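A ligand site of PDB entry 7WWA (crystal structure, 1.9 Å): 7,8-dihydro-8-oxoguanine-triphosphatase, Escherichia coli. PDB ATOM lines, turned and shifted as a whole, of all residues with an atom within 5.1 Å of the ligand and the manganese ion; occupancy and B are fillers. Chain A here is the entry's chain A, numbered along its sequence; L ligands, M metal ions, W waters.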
ATOM      1  N   ILE A   6      -0.930 -30.047  24.703  1.00  0.00           N
ATOM      2  CA  ILE A   6      -1.463 -29.045  25.626  1.00  0.00           C
ATOM      3  C   ILE A   6      -0.736 -29.183  26.960  1.00  0.00           C
ATOM      4  O   ILE A   6      -0.600 -30.287  27.485  1.00  0.00           O
ATOM      5  CB  ILE A   6      -2.979 -29.217  25.822  1.00  0.00           C
ATOM      6  CG1 ILE A   6      -3.723 -29.204  24.476  1.00  0.00           C
ATOM      7  CG2 ILE A   6      -3.517 -28.148  26.791  1.00  0.00           C
ATOM      8  CD1 ILE A   6      -3.500 -27.930  23.639  1.00  0.00           C
ATOM      9  N   VAL A   8      -0.840 -27.892  30.937  1.00  0.00           N
ATOM     10  CA  VAL A   8      -1.700 -27.268  31.943  1.00  0.00           C
ATOM     11  C   VAL A   8      -1.036 -27.394  33.311  1.00  0.00           C
ATOM     12  O   VAL A   8      -0.216 -28.281  33.566  1.00  0.00           O
ATOM     13  CB  VAL A   8      -3.124 -27.883  31.950  1.00  0.00           C
ATOM     14  CG1 VAL A   8      -3.674 -28.033  30.539  1.00  0.00           C
ATOM     15  CG2 VAL A   8      -3.157 -29.209  32.687  1.00  0.00           C
ATOM     16  N   ARG A  23     -13.860 -22.235  31.354  1.00  0.00           N
ATOM     17  CA  ARG A  23     -13.672 -21.946  29.941  1.00  0.00           C
ATOM     18  C   ARG A  23     -14.851 -21.157  29.389  1.00  0.00           C
ATOM     19  O   ARG A  23     -15.983 -21.262  29.872  1.00  0.00           O
ATOM     20  CB  ARG A  23     -13.480 -23.251  29.165  1.00  0.00           C
ATOM     21  CG  ARG A  23     -12.280 -24.026  29.661  1.00  0.00           C
ATOM     22  CD  ARG A  23     -12.037 -25.317  28.902  1.00  0.00           C
ATOM     23  NE  ARG A  23     -11.896 -25.113  27.470  1.00  0.00           N
ATOM     24  CZ  ARG A  23     -10.772 -24.748  26.866  1.00  0.00           C
ATOM     25  NH1 ARG A  23      -9.674 -24.520  27.570  1.00  0.00           N
ATOM     26  NH2 ARG A  23     -10.762 -24.588  25.551  1.00  0.00           N
ATOM     27  N   HIS A  28     -13.778 -24.573  22.633  1.00  0.00           N
ATOM     28  CA  HIS A  28     -13.826 -26.026  22.769  1.00  0.00           C
ATOM     29  C   HIS A  28     -13.971 -26.349  24.258  1.00  0.00           C
ATOM     30  O   HIS A  28     -13.412 -25.646  25.104  1.00  0.00           O
ATOM     31  CB  HIS A  28     -12.550 -26.663  22.198  1.00  0.00           C
ATOM     32  CG  HIS A  28     -12.573 -28.162  22.200  1.00  0.00           C
ATOM     33  ND1 HIS A  28     -11.747 -28.920  23.001  1.00  0.00           N
ATOM     34  CD2 HIS A  28     -13.371 -29.043  21.548  1.00  0.00           C
ATOM     35  CE1 HIS A  28     -12.013 -30.205  22.820  1.00  0.00           C
ATOM     36  NE2 HIS A  28     -13.000 -30.305  21.944  1.00  0.00           N
ATOM     37  N   MET A  29     -14.754 -27.372  24.578  1.00  0.00           N
ATOM     38  CA  MET A  29     -15.053 -27.712  25.973  1.00  0.00           C
ATOM     39  C   MET A  29     -15.633 -26.485  26.699  1.00  0.00           C
ATOM     40  O   MET A  29     -15.184 -26.088  27.778  1.00  0.00           O
ATOM     41  CB  MET A  29     -13.813 -28.255  26.689  1.00  0.00           C
ATOM     42  CG  MET A  29     -13.444 -29.677  26.256  1.00  0.00           C
ATOM     43  SD  MET A  29     -14.767 -30.814  26.769  1.00  0.00           S
ATOM     44  CE  MET A  29     -15.487 -31.281  25.187  1.00  0.00           C
ATOM     45  N   GLU A  34     -11.413 -26.040  34.412  1.00  0.00           N
ATOM     46  CA  GLU A  34     -10.160 -26.420  33.768  1.00  0.00           C
ATOM     47  C   GLU A  34      -8.992 -26.065  34.666  1.00  0.00           C
ATOM     48  O   GLU A  34      -9.083 -25.189  35.533  1.00  0.00           O
ATOM     49  CB  GLU A  34     -10.006 -25.715  32.423  1.00  0.00           C
ATOM     50  CG  GLU A  34     -10.127 -24.191  32.529  1.00  0.00           C
ATOM     51  CD  GLU A  34      -9.516 -23.446  31.345  1.00  0.00           C
ATOM     52  OE1 GLU A  34      -9.098 -24.104  30.350  1.00  0.00           O
ATOM     53  OE2 GLU A  34      -9.446 -22.202  31.420  1.00  0.00           O
ATOM     54  N   PHE A  35      -7.883 -26.765  34.441  1.00  0.00           N
ATOM     55  CA  PHE A  35      -6.574 -26.275  34.863  1.00  0.00           C
ATOM     56  C   PHE A  35      -6.074 -25.274  33.837  1.00  0.00           C
ATOM     57  O   PHE A  35      -6.158 -25.537  32.623  1.00  0.00           O
ATOM     58  CB  PHE A  35      -5.588 -27.461  34.980  1.00  0.00           C
ATOM     59  CG  PHE A  35      -6.084 -28.580  35.865  1.00  0.00           C
ATOM     60  CD1 PHE A  35      -6.401 -28.338  37.200  1.00  0.00           C
ATOM     61  CD2 PHE A  35      -6.240 -29.863  35.356  1.00  0.00           C
ATOM     62  CE1 PHE A  35      -6.868 -29.369  38.017  1.00  0.00           C
ATOM     63  CE2 PHE A  35      -6.696 -30.891  36.161  1.00  0.00           C
ATOM     64  CZ  PHE A  35      -7.021 -30.655  37.495  1.00  0.00           C
ATOM     65  N   PRO A  36      -5.571 -24.102  34.242  1.00  0.00           N
ATOM     66  CA  PRO A  36      -5.066 -23.162  33.243  1.00  0.00           C
ATOM     67  C   PRO A  36      -3.962 -23.801  32.416  1.00  0.00           C
ATOM     68  O   PRO A  36      -3.164 -24.597  32.930  1.00  0.00           O
ATOM     69  CB  PRO A  36      -4.533 -21.994  34.098  1.00  0.00           C
ATOM     70  CG  PRO A  36      -5.366 -22.075  35.365  1.00  0.00           C
ATOM     71  CD  PRO A  36      -5.522 -23.550  35.611  1.00  0.00           C
ATOM     72  N   GLY A  37      -3.937 -23.497  31.123  1.00  0.00           N
ATOM     73  CA  GLY A  37      -2.957 -24.099  30.246  1.00  0.00           C
ATOM     74  C   GLY A  37      -3.295 -23.793  28.799  1.00  0.00           C
ATOM     75  O   GLY A  37      -4.188 -23.005  28.515  1.00  0.00           O
ATOM     76  N   GLY A  38      -2.554 -24.407  27.889  1.00  0.00           N
ATOM     77  CA  GLY A  38      -2.771 -24.151  26.487  1.00  0.00           C
ATOM     78  C   GLY A  38      -1.748 -24.862  25.624  1.00  0.00           C
ATOM     79  O   GLY A  38      -0.949 -25.655  26.115  1.00  0.00           O
ATOM     80  N   LYS A  39      -1.772 -24.528  24.337  1.00  0.00           N
ATOM     81  CA  LYS A  39      -1.002 -25.284  23.347  1.00  0.00           C
ATOM     82  C   LYS A  39       0.495 -25.039  23.502  1.00  0.00           C
ATOM     83  O   LYS A  39       0.944 -23.895  23.678  1.00  0.00           O
ATOM     84  CB  LYS A  39      -1.444 -24.895  21.935  1.00  0.00           C
ATOM     85  CG  LYS A  39      -0.705 -25.663  20.844  1.00  0.00           C
ATOM     86  CD  LYS A  39      -0.918 -25.051  19.471  1.00  0.00           C
ATOM     87  CE  LYS A  39       0.050 -25.666  18.452  1.00  0.00           C
ATOM     88  NZ  LYS A  39       0.029 -24.967  17.140  1.00  0.00           N
ATOM     89  N   GLU A  53       2.037 -20.335  29.668  1.00  0.00           N
ATOM     90  CA  GLU A  53       0.576 -20.345  29.746  1.00  0.00           C
ATOM     91  C   GLU A  53       0.063 -19.831  31.098  1.00  0.00           C
ATOM     92  O   GLU A  53      -0.924 -19.101  31.155  1.00  0.00           O
ATOM     93  CB  GLU A  53       0.045 -21.748  29.463  1.00  0.00           C
ATOM     94  CG  GLU A  53       0.160 -22.171  28.000  1.00  0.00           C
ATOM     95  CD  GLU A  53      -0.822 -21.425  27.097  1.00  0.00           C
ATOM     96  OE1 GLU A  53      -1.820 -20.883  27.627  1.00  0.00           O
ATOM     97  OE2 GLU A  53      -0.604 -21.372  25.879  1.00  0.00           O
ATOM     98  N   GLU A  57      -2.338 -16.670  31.502  1.00  0.00           N
ATOM     99  CA  GLU A  57      -3.729 -16.864  31.872  1.00  0.00           C
ATOM    100  C   GLU A  57      -4.025 -16.397  33.291  1.00  0.00           C
ATOM    101  O   GLU A  57      -5.112 -15.862  33.542  1.00  0.00           O
ATOM    102  CB  GLU A  57      -4.124 -18.335  31.736  1.00  0.00           C
ATOM    103  CG  GLU A  57      -4.008 -18.833  30.316  1.00  0.00           C
ATOM    104  CD  GLU A  57      -4.986 -19.921  29.989  1.00  0.00           C
ATOM    105  OE1 GLU A  57      -5.454 -20.631  30.899  1.00  0.00           O
ATOM    106  OE2 GLU A  57      -5.301 -20.046  28.792  1.00  0.00           O
ATOM    107  N   PHE A  75     -11.116 -36.430  21.344  1.00  0.00           N
ATOM    108  CA  PHE A  75     -12.386 -35.714  21.321  1.00  0.00           C
ATOM    109  C   PHE A  75     -13.088 -35.974  19.988  1.00  0.00           C
ATOM    110  O   PHE A  75     -12.478 -36.460  19.039  1.00  0.00           O
ATOM    111  CB  PHE A  75     -12.152 -34.222  21.511  1.00  0.00           C
ATOM    112  CG  PHE A  75     -11.803 -33.836  22.899  1.00  0.00           C
ATOM    113  CD1 PHE A  75     -12.789 -33.688  23.861  1.00  0.00           C
ATOM    114  CD2 PHE A  75     -10.490 -33.575  23.251  1.00  0.00           C
ATOM    115  CE1 PHE A  75     -12.479 -33.304  25.167  1.00  0.00           C
ATOM    116  CE2 PHE A  75     -10.164 -33.177  24.536  1.00  0.00           C
ATOM    117  CZ  PHE A  75     -11.158 -33.052  25.500  1.00  0.00           C
ATOM    118  N   ARG A  78     -10.997 -33.705  17.511  1.00  0.00           N
ATOM    119  CA  ARG A  78      -9.591 -33.390  17.669  1.00  0.00           C
ATOM    120  C   ARG A  78      -8.957 -34.383  18.634  1.00  0.00           C
ATOM    121  O   ARG A  78      -9.631 -34.949  19.499  1.00  0.00           O
ATOM    122  CB  ARG A  78      -9.385 -31.955  18.171  1.00  0.00           C
ATOM    123  CG  ARG A  78      -9.895 -31.701  19.575  1.00  0.00           C
ATOM    124  CD  ARG A  78     -10.017 -30.198  19.833  1.00  0.00           C
ATOM    125  NE  ARG A  78     -11.092 -29.625  19.018  1.00  0.00           N
ATOM    126  CZ  ARG A  78     -11.259 -28.326  18.805  1.00  0.00           C
ATOM    127  NH1 ARG A  78     -10.415 -27.452  19.314  1.00  0.00           N
ATOM    128  NH2 ARG A  78     -12.270 -27.899  18.061  1.00  0.00           N
ATOM    129  N   ILE A  80      -5.836 -34.681  21.404  1.00  0.00           N
ATOM    130  CA  ILE A  80      -4.886 -33.882  22.158  1.00  0.00           C
ATOM    131  C   ILE A  80      -4.093 -34.753  23.118  1.00  0.00           C
ATOM    132  O   ILE A  80      -4.577 -35.767  23.626  1.00  0.00           O
ATOM    133  CB  ILE A  80      -5.554 -32.713  22.924  1.00  0.00           C
ATOM    134  CG1 ILE A  80      -6.314 -33.231  24.136  1.00  0.00           C
ATOM    135  CG2 ILE A  80      -6.435 -31.868  22.021  1.00  0.00           C
ATOM    136  CD1 ILE A  80      -6.753 -32.099  25.029  1.00  0.00           C
ATOM    137  N   LEU A  82      -2.276 -34.242  26.681  1.00  0.00           N
ATOM    138  CA  LEU A  82      -2.306 -33.299  27.794  1.00  0.00           C
ATOM    139  C   LEU A  82      -1.142 -33.558  28.731  1.00  0.00           C
ATOM    140  O   LEU A  82      -0.935 -34.694  29.176  1.00  0.00           O
ATOM    141  CB  LEU A  82      -3.629 -33.409  28.557  1.00  0.00           C
ATOM    142  CG  LEU A  82      -4.793 -32.634  27.960  1.00  0.00           C
ATOM    143  CD1 LEU A  82      -6.101 -33.315  28.294  1.00  0.00           C
ATOM    144  CD2 LEU A  82      -4.810 -31.193  28.503  1.00  0.00           C
ATOM    145  N   PHE A  84      -0.031 -32.636  32.334  1.00  0.00           N
ATOM    146  CA  PHE A  84      -0.566 -32.111  33.582  1.00  0.00           C
ATOM    147  C   PHE A  84       0.598 -31.894  34.561  1.00  0.00           C
ATOM    148  O   PHE A  84       1.132 -32.875  35.088  1.00  0.00           O
ATOM    149  CB  PHE A  84      -1.582 -33.070  34.204  1.00  0.00           C
ATOM    150  CG  PHE A  84      -2.862 -33.230  33.423  1.00  0.00           C
ATOM    151  CD1 PHE A  84      -3.954 -32.407  33.682  1.00  0.00           C
ATOM    152  CD2 PHE A  84      -2.980 -34.232  32.469  1.00  0.00           C
ATOM    153  CE1 PHE A  84      -5.146 -32.559  32.972  1.00  0.00           C
ATOM    154  CE2 PHE A  84      -4.158 -34.403  31.758  1.00  0.00           C
ATOM    155  CZ  PHE A  84      -5.253 -33.558  32.005  1.00  0.00           C
ATOM    156  N   PRO A 116     -13.386 -31.228  31.390  1.00  0.00           N
ATOM    157  CA  PRO A 116     -13.377 -32.045  30.184  1.00  0.00           C
ATOM    158  C   PRO A 116     -13.159 -33.500  30.546  1.00  0.00           C
ATOM    159  O   PRO A 116     -12.487 -33.818  31.551  1.00  0.00           O
ATOM    160  CB  PRO A 116     -12.211 -31.489  29.365  1.00  0.00           C
ATOM    161  CG  PRO A 116     -12.090 -30.056  29.855  1.00  0.00           C
ATOM    162  CD  PRO A 116     -12.354 -30.171  31.330  1.00  0.00           C
ATOM    163  N   ALA A 118     -11.297 -35.696  29.425  1.00  0.00           N
ATOM    164  CA  ALA A 118      -9.898 -36.098  29.433  1.00  0.00           C
ATOM    165  C   ALA A 118      -9.283 -35.998  30.824  1.00  0.00           C
ATOM    166  O   ALA A 118      -8.339 -36.737  31.119  1.00  0.00           O
ATOM    167  CB  ALA A 118      -9.096 -35.236  28.452  1.00  0.00           C
ATOM    168  N   ASN A 119      -9.804 -35.117  31.683  1.00  0.00           N
ATOM    169  CA  ASN A 119      -9.259 -34.916  33.017  1.00  0.00           C
ATOM    170  C   ASN A 119      -9.668 -35.987  34.041  1.00  0.00           C
ATOM    171  O   ASN A 119      -9.139 -35.982  35.155  1.00  0.00           O
ATOM    172  CB  ASN A 119      -9.675 -33.547  33.551  1.00  0.00           C
ATOM    173  CG  ASN A 119      -9.084 -32.400  32.758  1.00  0.00           C
ATOM    174  OD1 ASN A 119      -8.774 -32.539  31.581  1.00  0.00           O
ATOM    175  ND2 ASN A 119      -8.914 -31.256  33.413  1.00  0.00           N
HETATM  176  O1  LIG L   1      -8.319 -23.668  24.592  1.00  0.00           O
HETATM  177  P1  LIG L   1      -6.867 -23.843  24.964  1.00  0.00           P
HETATM  178  O2  LIG L   1      -5.862 -23.046  24.183  1.00  0.00           O
HETATM  179  O3  LIG L   1      -6.659 -23.801  26.459  1.00  0.00           O
HETATM  180  O4  LIG L   1      -6.547 -25.374  24.582  1.00  0.00           O
HETATM  181  C1  LIG L   1      -6.729 -26.403  25.542  1.00  0.00           C
HETATM  182  C2  LIG L   1      -7.296 -27.671  24.887  1.00  0.00           C
HETATM  183  O5  LIG L   1      -7.080 -28.737  25.801  1.00  0.00           O
HETATM  184  C3  LIG L   1      -8.802 -27.597  24.675  1.00  0.00           C
HETATM  185  O6  LIG L   1      -9.159 -28.465  23.588  1.00  0.00           O
HETATM  186  C4  LIG L   1      -9.384 -28.224  25.934  1.00  0.00           C
HETATM  187  C5  LIG L   1      -8.323 -29.259  26.279  1.00  0.00           C
HETATM  188  N1  LIG L   1      -8.265 -29.432  27.753  1.00  0.00           N
HETATM  189  C6  LIG L   1      -8.642 -30.483  28.456  1.00  0.00           C
HETATM  190  N2  LIG L   1      -8.473 -30.382  29.784  1.00  0.00           N
HETATM  191  C7  LIG L   1      -7.938 -29.132  29.933  1.00  0.00           C
HETATM  192  C8  LIG L   1      -7.536 -28.411  31.048  1.00  0.00           C
HETATM  193  O7  LIG L   1      -7.663 -28.909  32.202  1.00  0.00           O
HETATM  194  N3  LIG L   1      -7.030 -27.175  30.875  1.00  0.00           N
HETATM  195  C9  LIG L   1      -6.914 -26.636  29.652  1.00  0.00           C
HETATM  196  N4  LIG L   1      -6.395 -25.401  29.475  1.00  0.00           N
HETATM  197  N5  LIG L   1      -7.288 -27.313  28.551  1.00  0.00           N
HETATM  198  C10 LIG L   1      -7.805 -28.560  28.664  1.00  0.00           C
HETATM  199  O8  LIG L   1      -9.127 -31.524  27.892  1.00  0.00           O
HETATM  200 MN    MN M   1      -6.030 -22.003  27.708  1.00  0.00          MN
HETATM  201  O   HOH W   1      -6.522 -21.195  22.584  1.00  0.00           O
HETATM  202  O   HOH W   2      -8.027 -20.629  27.360  1.00  0.00           O
HETATM  203  O   HOH W   3      -6.955 -22.632  29.807  1.00  0.00           O
HETATM  204  O   HOH W   4      -9.088 -24.646  22.054  1.00  0.00           O
HETATM  205  O   HOH W   5      -9.443 -21.352  25.390  1.00  0.00           O
HETATM  206  O   HOH W   6      -5.135 -21.243  25.661  1.00  0.00           O
HETATM  207  O   HOH W   7      -8.382 -27.260  21.267  1.00  0.00           O
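The backbone NH (N) of Phe 35 lies within hydrogen-bond range of an oxygen (O7) of the ligand (3.1 Å). A nitrogen (N3) of the ligand is in hydrogen-bond range of the backbone carbonyl oxygen (O) of Phe 35. An oxygen (O6) of the ligand is in hydrogen-bond range of a ring nitrogen (ND1) of His 28. NH2 of Arg 23 is in salt-bridge range of O1 of the ligand. N2 of the ligand is in hydrogen-bond range of OD1 of Asn 119. A nitrogen (N4) of the ligand lies within hydrogen-bond range of the side-chain carboxylate (OE1) of Glu 34 (3.1 Å).
The backbone carbonyl oxygen (O) of His 28 lies within hydrogen-bond range of the guanidinium group (NE) of Arg 23 (2.9 Å). The side-chain carboxylate of Glu 34 lies within salt-bridge range of the guanidinium group of Arg 23. The backbone carbonyl oxygen (O) of Met 29 sits close to the guanidinium group (NE) of Arg 23 (3.4 Å).
Ile 6 touches the ligand (CG1 to O5, 3.6 Å). Val 8 touches the ligand. Gly 38 touches the ligand. Phe 75 touches the ligand. Ile 80 touches the ligand. Leu 82 touches the ligand (CD1 to O8, 3.5 Å). Pro 116 touches the ligand. CB of Ala 118 touches O8 of the ligand, at 3.8 Å. Hydrophobic or aromatic side chains that line the ligand: Ile 6, Val 8, His 28, Phe 35, Phe 75, Ile 80, Leu 82, Pro 116 and Ala 118. Within 4 Å of the ligand: Ile 6, Val 8, Arg 23, His 28, Glu 34, Phe 35, Gly 37, Gly 38, Phe 75, Ile 80, Leu 82, Pro 116, Ala 118 and Asn 119.
Within 4 Å of the manganese ion: Gly 37 and Glu 57.
The manganese ion is bound by O of Gly 37, O3 of the ligand, OE2 of Glu 57, water W6, water W3 and water W2.
Water W3 lies within hydrogen-bond range of OE1 of Glu 34 (2.7 Å), OE1 of Glu 57 (2.7 Å), N4 of the ligand (2.8 Å) and N of Gly 37 (3.4 Å). Water W5 lies within hydrogen-bond range of an oxygen (O1) of the ligand (2.7 Å) and the guanidinium group of Arg 23 (3.5 Å). Water W7 lies within hydrogen-bond range of an oxygen (O6) of the ligand and the guanidinium group (NH1) of Arg 78.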
